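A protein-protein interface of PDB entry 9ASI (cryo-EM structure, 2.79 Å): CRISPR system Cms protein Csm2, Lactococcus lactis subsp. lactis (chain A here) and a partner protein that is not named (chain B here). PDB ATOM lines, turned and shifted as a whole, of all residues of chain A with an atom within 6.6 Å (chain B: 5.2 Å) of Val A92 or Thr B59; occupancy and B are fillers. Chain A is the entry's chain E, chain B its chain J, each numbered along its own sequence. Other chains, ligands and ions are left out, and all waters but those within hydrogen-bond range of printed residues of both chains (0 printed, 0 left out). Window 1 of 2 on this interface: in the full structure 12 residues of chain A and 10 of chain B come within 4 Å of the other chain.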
ATOM      1  N   ILE A  87      -3.334 -16.862  27.432  1.00  0.00           N
ATOM      2  CA  ILE A  87      -3.913 -16.105  28.539  1.00  0.00           C
ATOM      3  C   ILE A  87      -2.915 -15.077  29.065  1.00  0.00           C
ATOM      4  O   ILE A  87      -3.290 -13.964  29.458  1.00  0.00           O
ATOM      5  CB  ILE A  87      -4.388 -17.064  29.647  1.00  0.00           C
ATOM      6  CG1 ILE A  87      -5.525 -17.950  29.129  1.00  0.00           C
ATOM      7  CG2 ILE A  87      -4.836 -16.292  30.877  1.00  0.00           C
ATOM      8  CD1 ILE A  87      -6.289 -18.675  30.216  1.00  0.00           C
ATOM      9  N   ALA A  88      -1.628 -15.429  29.074  1.00  0.00           N
ATOM     10  CA  ALA A  88      -0.605 -14.466  29.470  1.00  0.00           C
ATOM     11  C   ALA A  88      -0.567 -13.279  28.515  1.00  0.00           C
ATOM     12  O   ALA A  88      -0.461 -12.124  28.947  1.00  0.00           O
ATOM     13  CB  ALA A  88       0.759 -15.151  29.529  1.00  0.00           C
ATOM     14  N   TYR A  89      -0.655 -13.543  27.212  1.00  0.00           N
ATOM     15  CA  TYR A  89      -0.710 -12.455  26.244  1.00  0.00           C
ATOM     16  C   TYR A  89      -1.997 -11.650  26.386  1.00  0.00           C
ATOM     17  O   TYR A  89      -1.997 -10.435  26.155  1.00  0.00           O
ATOM     18  CB  TYR A  89      -0.570 -13.006  24.827  1.00  0.00           C
ATOM     19  CG  TYR A  89      -0.195 -11.959  23.805  1.00  0.00           C
ATOM     20  CD1 TYR A  89       1.007 -11.273  23.894  1.00  0.00           C
ATOM     21  CD2 TYR A  89      -1.045 -11.660  22.750  1.00  0.00           C
ATOM     22  CE1 TYR A  89       1.352 -10.317  22.963  1.00  0.00           C
ATOM     23  CE2 TYR A  89      -0.709 -10.705  21.814  1.00  0.00           C
ATOM     24  CZ  TYR A  89       0.490 -10.037  21.924  1.00  0.00           C
ATOM     25  OH  TYR A  89       0.824  -9.084  20.991  1.00  0.00           O
ATOM     26  N   ILE A  90      -3.095 -12.308  26.768  1.00  0.00           N
ATOM     27  CA  ILE A  90      -4.321 -11.592  27.109  1.00  0.00           C
ATOM     28  C   ILE A  90      -4.045 -10.587  28.217  1.00  0.00           C
ATOM     29  O   ILE A  90      -4.432  -9.416  28.133  1.00  0.00           O
ATOM     30  CB  ILE A  90      -5.427 -12.579  27.525  1.00  0.00           C
ATOM     31  CG1 ILE A  90      -6.149 -13.154  26.308  1.00  0.00           C
ATOM     32  CG2 ILE A  90      -6.424 -11.914  28.467  1.00  0.00           C
ATOM     33  CD1 ILE A  90      -7.079 -14.296  26.660  1.00  0.00           C
ATOM     34  N   LYS A  91      -3.369 -11.040  29.274  1.00  0.00           N
ATOM     35  CA  LYS A  91      -3.060 -10.154  30.392  1.00  0.00           C
ATOM     36  C   LYS A  91      -2.150  -9.014  29.953  1.00  0.00           C
ATOM     37  O   LYS A  91      -2.299  -7.878  30.419  1.00  0.00           O
ATOM     38  CB  LYS A  91      -2.428 -10.945  31.536  1.00  0.00           C
ATOM     39  CG  LYS A  91      -2.321 -10.170  32.841  1.00  0.00           C
ATOM     40  CD  LYS A  91      -2.321 -11.096  34.045  1.00  0.00           C
ATOM     41  CE  LYS A  91      -2.276 -10.312  35.346  1.00  0.00           C
ATOM     42  NZ  LYS A  91      -3.281  -9.216  35.372  1.00  0.00           N
ATOM     43  N   VAL A  92      -1.198  -9.297  29.058  1.00  0.00           N
ATOM     44  CA  VAL A  92      -0.324  -8.242  28.539  1.00  0.00           C
ATOM     45  C   VAL A  92      -1.143  -7.181  27.814  1.00  0.00           C
ATOM     46  O   VAL A  92      -0.971  -5.973  28.031  1.00  0.00           O
ATOM     47  CB  VAL A  92       0.754  -8.833  27.611  1.00  0.00           C
ATOM     48  CG1 VAL A  92       1.627  -7.722  27.049  1.00  0.00           C
ATOM     49  CG2 VAL A  92       1.601  -9.844  28.345  1.00  0.00           C
ATOM     50  N   LYS A  93      -2.043  -7.623  26.933  1.00  0.00           N
ATOM     51  CA  LYS A  93      -2.871  -6.685  26.185  1.00  0.00           C
ATOM     52  C   LYS A  93      -3.745  -5.861  27.119  1.00  0.00           C
ATOM     53  O   LYS A  93      -3.892  -4.648  26.934  1.00  0.00           O
ATOM     54  CB  LYS A  93      -3.739  -7.437  25.176  1.00  0.00           C
ATOM     55  CG  LYS A  93      -2.995  -8.259  24.129  1.00  0.00           C
ATOM     56  CD  LYS A  93      -2.304  -7.405  23.079  1.00  0.00           C
ATOM     57  CE  LYS A  93      -0.837  -7.175  23.401  1.00  0.00           C
ATOM     58  NZ  LYS A  93      -0.154  -6.453  22.299  1.00  0.00           N
ATOM     59  N   ILE A  94      -4.337  -6.507  28.127  1.00  0.00           N
ATOM     60  CA  ILE A  94      -5.206  -5.795  29.057  1.00  0.00           C
ATOM     61  C   ILE A  94      -4.413  -4.773  29.855  1.00  0.00           C
ATOM     62  O   ILE A  94      -4.874  -3.649  30.078  1.00  0.00           O
ATOM     63  CB  ILE A  94      -5.940  -6.784  29.980  1.00  0.00           C
ATOM     64  CG1 ILE A  94      -6.763  -7.768  29.152  1.00  0.00           C
ATOM     65  CG2 ILE A  94      -6.828  -6.041  30.962  1.00  0.00           C
ATOM     66  CD1 ILE A  94      -7.618  -7.117  28.114  1.00  0.00           C
ATOM     67  N   ALA A  95      -3.211  -5.145  30.306  1.00  0.00           N
ATOM     68  CA  ALA A  95      -2.378  -4.206  31.047  1.00  0.00           C
ATOM     69  C   ALA A  95      -2.019  -3.000  30.192  1.00  0.00           C
ATOM     70  O   ALA A  95      -2.100  -1.856  30.656  1.00  0.00           O
ATOM     71  CB  ALA A  95      -1.115  -4.905  31.546  1.00  0.00           C
ATOM     72  N   TYR A  96      -1.636  -3.232  28.934  1.00  0.00           N
ATOM     73  CA  TYR A  96      -1.297  -2.115  28.057  1.00  0.00           C
ATOM     74  C   TYR A  96      -2.505  -1.216  27.814  1.00  0.00           C
ATOM     75  O   TYR A  96      -2.404   0.015  27.888  1.00  0.00           O
ATOM     76  CB  TYR A  96      -0.742  -2.632  26.731  1.00  0.00           C
ATOM     77  CG  TYR A  96      -0.692  -1.575  25.650  1.00  0.00           C
ATOM     78  CD1 TYR A  96      -0.056  -0.360  25.870  1.00  0.00           C
ATOM     79  CD2 TYR A  96      -1.289  -1.787  24.416  1.00  0.00           C
ATOM     80  CE1 TYR A  96      -0.014   0.612  24.892  1.00  0.00           C
ATOM     81  CE2 TYR A  96      -1.248  -0.821  23.430  1.00  0.00           C
ATOM     82  CZ  TYR A  96      -0.608   0.375  23.673  1.00  0.00           C
ATOM     83  OH  TYR A  96      -0.566   1.339  22.694  1.00  0.00           O
ATOM     84  N   GLU A  97      -3.662  -1.817  27.525  1.00  0.00           N
ATOM     85  CA  GLU A  97      -4.850  -1.023  27.227  1.00  0.00           C
ATOM     86  C   GLU A  97      -5.305  -0.227  28.444  1.00  0.00           C
ATOM     87  O   GLU A  97      -5.753   0.917  28.311  1.00  0.00           O
ATOM     88  CB  GLU A  97      -5.973  -1.924  26.717  1.00  0.00           C
ATOM     89  CG  GLU A  97      -5.891  -2.229  25.226  1.00  0.00           C
ATOM     90  CD  GLU A  97      -5.986  -0.983  24.360  1.00  0.00           C
ATOM     91  OE1 GLU A  97      -6.554   0.030  24.821  1.00  0.00           O
ATOM     92  OE2 GLU A  97      -5.491  -1.018  23.213  1.00  0.00           O
ATOM     93  N   TYR B  26       4.628  -5.533  20.516  1.00  0.00           N
ATOM     94  CA  TYR B  26       4.570  -6.366  21.705  1.00  0.00           C
ATOM     95  C   TYR B  26       4.733  -7.845  21.408  1.00  0.00           C
ATOM     96  O   TYR B  26       5.004  -8.615  22.336  1.00  0.00           O
ATOM     97  CB  TYR B  26       3.249  -6.141  22.454  1.00  0.00           C
ATOM     98  CG  TYR B  26       3.019  -4.692  22.798  1.00  0.00           C
ATOM     99  CD1 TYR B  26       4.064  -3.899  23.242  1.00  0.00           C
ATOM    100  CD2 TYR B  26       1.772  -4.108  22.650  1.00  0.00           C
ATOM    101  CE1 TYR B  26       3.869  -2.572  23.548  1.00  0.00           C
ATOM    102  CE2 TYR B  26       1.567  -2.780  22.952  1.00  0.00           C
ATOM    103  CZ  TYR B  26       2.621  -2.016  23.400  1.00  0.00           C
ATOM    104  OH  TYR B  26       2.431  -0.689  23.704  1.00  0.00           O
ATOM    105  N   LEU B  54       8.973 -16.288  33.822  1.00  0.00           N
ATOM    106  CA  LEU B  54       7.574 -16.658  33.943  1.00  0.00           C
ATOM    107  C   LEU B  54       6.678 -15.667  33.204  1.00  0.00           C
ATOM    108  O   LEU B  54       7.044 -14.515  32.946  1.00  0.00           O
ATOM    109  CB  LEU B  54       7.168 -16.745  35.413  1.00  0.00           C
ATOM    110  CG  LEU B  54       7.370 -18.104  36.087  1.00  0.00           C
ATOM    111  CD1 LEU B  54       7.047 -18.023  37.570  1.00  0.00           C
ATOM    112  CD2 LEU B  54       6.530 -19.175  35.408  1.00  0.00           C
ATOM    113  N   LEU B  55       5.477 -16.142  32.866  1.00  0.00           N
ATOM    114  CA  LEU B  55       4.573 -15.373  32.016  1.00  0.00           C
ATOM    115  C   LEU B  55       4.045 -14.131  32.728  1.00  0.00           C
ATOM    116  O   LEU B  55       3.874 -13.080  32.102  1.00  0.00           O
ATOM    117  CB  LEU B  55       3.421 -16.263  31.553  1.00  0.00           C
ATOM    118  CG  LEU B  55       3.774 -17.721  31.245  1.00  0.00           C
ATOM    119  CD1 LEU B  55       2.524 -18.507  30.881  1.00  0.00           C
ATOM    120  CD2 LEU B  55       4.809 -17.809  30.131  1.00  0.00           C
ATOM    121  N   ASP B  56       3.768 -14.231  34.030  1.00  0.00           N
ATOM    122  CA  ASP B  56       3.310 -13.058  34.771  1.00  0.00           C
ATOM    123  C   ASP B  56       4.395 -11.989  34.843  1.00  0.00           C
ATOM    124  O   ASP B  56       4.107 -10.791  34.721  1.00  0.00           O
ATOM    125  CB  ASP B  56       2.851 -13.465  36.171  1.00  0.00           C
ATOM    126  CG  ASP B  56       3.850 -14.359  36.876  1.00  0.00           C
ATOM    127  OD1 ASP B  56       4.901 -14.668  36.276  1.00  0.00           O
ATOM    128  OD2 ASP B  56       3.584 -14.756  38.030  1.00  0.00           O
ATOM    129  N   ASP B  57       5.648 -12.402  35.054  1.00  0.00           N
ATOM    130  CA  ASP B  57       6.755 -11.452  35.031  1.00  0.00           C
ATOM    131  C   ASP B  57       6.914 -10.835  33.647  1.00  0.00           C
ATOM    132  O   ASP B  57       7.244  -9.650  33.521  1.00  0.00           O
ATOM    133  CB  ASP B  57       8.046 -12.144  35.467  1.00  0.00           C
ATOM    134  CG  ASP B  57       9.117 -11.162  35.899  1.00  0.00           C
ATOM    135  OD1 ASP B  57       8.834  -9.946  35.930  1.00  0.00           O
ATOM    136  OD2 ASP B  57      10.242 -11.607  36.208  1.00  0.00           O
ATOM    137  N   PHE B  58       6.692 -11.630  32.598  1.00  0.00           N
ATOM    138  CA  PHE B  58       6.678 -11.089  31.242  1.00  0.00           C
ATOM    139  C   PHE B  58       5.604 -10.017  31.098  1.00  0.00           C
ATOM    140  O   PHE B  58       5.839  -8.954  30.510  1.00  0.00           O
ATOM    141  CB  PHE B  58       6.448 -12.223  30.239  1.00  0.00           C
ATOM    142  CG  PHE B  58       6.613 -11.815  28.801  1.00  0.00           C
ATOM    143  CD1 PHE B  58       5.547 -11.288  28.089  1.00  0.00           C
ATOM    144  CD2 PHE B  58       7.824 -11.986  28.153  1.00  0.00           C
ATOM    145  CE1 PHE B  58       5.694 -10.919  26.765  1.00  0.00           C
ATOM    146  CE2 PHE B  58       7.978 -11.621  26.828  1.00  0.00           C
ATOM    147  CZ  PHE B  58       6.911 -11.088  26.133  1.00  0.00           C
ATOM    148  N   THR B  59       4.413 -10.288  31.632  1.00  0.00           N
ATOM    149  CA  THR B  59       3.291  -9.365  31.491  1.00  0.00           C
ATOM    150  C   THR B  59       3.528  -8.063  32.246  1.00  0.00           C
ATOM    151  O   THR B  59       3.231  -6.977  31.734  1.00  0.00           O
ATOM    152  CB  THR B  59       2.005 -10.024  31.990  1.00  0.00           C
ATOM    153  OG1 THR B  59       1.727 -11.196  31.213  1.00  0.00           O
ATOM    154  CG2 THR B  59       0.845  -9.055  31.881  1.00  0.00           C
ATOM    155  N   SER B  60       4.067  -8.151  33.462  1.00  0.00           N
ATOM    156  CA  SER B  60       4.103  -7.008  34.369  1.00  0.00           C
ATOM    157  C   SER B  60       5.040  -5.890  33.924  1.00  0.00           C
ATOM    158  O   SER B  60       5.175  -4.905  34.661  1.00  0.00           O
ATOM    159  CB  SER B  60       4.496  -7.477  35.773  1.00  0.00           C
ATOM    160  OG  SER B  60       5.795  -8.045  35.778  1.00  0.00           O
ATOM    161  N   ARG B  61       5.680  -5.990  32.758  1.00  0.00           N
ATOM    162  CA  ARG B  61       6.665  -4.999  32.338  1.00  0.00           C
ATOM    163  C   ARG B  61       6.262  -4.290  31.047  1.00  0.00           C
ATOM    164  O   ARG B  61       7.118  -3.951  30.226  1.00  0.00           O
ATOM    165  CB  ARG B  61       8.045  -5.640  32.193  1.00  0.00           C
ATOM    166  CG  ARG B  61       8.144  -6.725  31.133  1.00  0.00           C
ATOM    167  CD  ARG B  61       9.598  -7.097  30.892  1.00  0.00           C
ATOM    168  NE  ARG B  61       9.787  -7.834  29.649  1.00  0.00           N
ATOM    169  CZ  ARG B  61       9.882  -9.153  29.566  1.00  0.00           C
ATOM    170  NH1 ARG B  61       9.799  -9.922  30.639  1.00  0.00           N
ATOM    171  NH2 ARG B  61      10.072  -9.716  28.376  1.00  0.00           N
ATOM    172  N   VAL B  62       4.970  -4.036  30.857  1.00  0.00           N
ATOM    173  CA  VAL B  62       4.480  -3.298  29.697  1.00  0.00           C
ATOM    174  C   VAL B  62       3.959  -1.945  30.169  1.00  0.00           C
ATOM    175  O   VAL B  62       3.057  -1.869  31.012  1.00  0.00           O
ATOM    176  CB  VAL B  62       3.408  -4.086  28.922  1.00  0.00           C
ATOM    177  CG1 VAL B  62       2.250  -4.497  29.827  1.00  0.00           C
ATOM    178  CG2 VAL B  62       2.910  -3.273  27.733  1.00  0.00           C
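O of Ala A88 is in hydrogen-bond range of OG1 of Thr B59 (3.3 Å).
Of the 11 printed residues of chain A, 6 touch a printed residue of chain B.
Printed residues of chain A that touch a printed residue of chain B: Ala A88, Lys A91, Val A92, Lys A93, Ala A95 and Tyr A96.
Hydrophobic or aromatic side chains of chain A within 4 Å of the printed part of chain B: Ala A88, Val A92, Ala A95 and Tyr A96.
Among the printed residues, 9 pairs touch across the chains.
Val A92 touches just these residues of chain B: Thr B59 (3.2 Å) and Val B62 (3.97 Å).
Thr B59 touches just these residues of chain A: Ala A88 (3.3 Å), Lys A91 (3.5 Å) and Val A92 (3.2 Å).
Of the printed residues of chain A, Leu B55 touches Ala A88 (3.5 Å).
Of the printed residues of chain B, Ala A88 touches Leu B55 and Thr B59.
Printed residues of chain A within 4 Å of Val B62: Val A92 (3.97 Å), Ala A95 (3.8 Å) and Tyr A96 (3.8 Å).
Of the printed residues of chain B, Tyr A96 touches Tyr B26 (3.0 Å) and Val B62 (3.8 Å).
The nearest residue of chain B that does not touch Val A92 is Phe B58 (4.2 Å).
CB of Ala A88 touches CB of Leu B55 (3.5 Å).
Thr B59 touches Lys A91.
OG1 of Thr B59 touches CG2 of Val A92 (3.2 Å).
O of Val A92 touches CG1 of Val B62, 3.97 Å away.
Tyr B26 touches Lys A93.
Val B62 touches Ala A95 (CG1 to CB, 3.8 Å).
Tyr A96 touches Tyr B26.
CB of Tyr A96 touches CG2 of Val B62, at 3.8 Å.
The side-chain hydroxyl of Tyr A89 is in hydrogen-bond range of the side-chain amino group of Lys A93 (3.1 Å).
OG1 of Thr B59 sits at hydrogen-bond distance from O of Leu B55.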
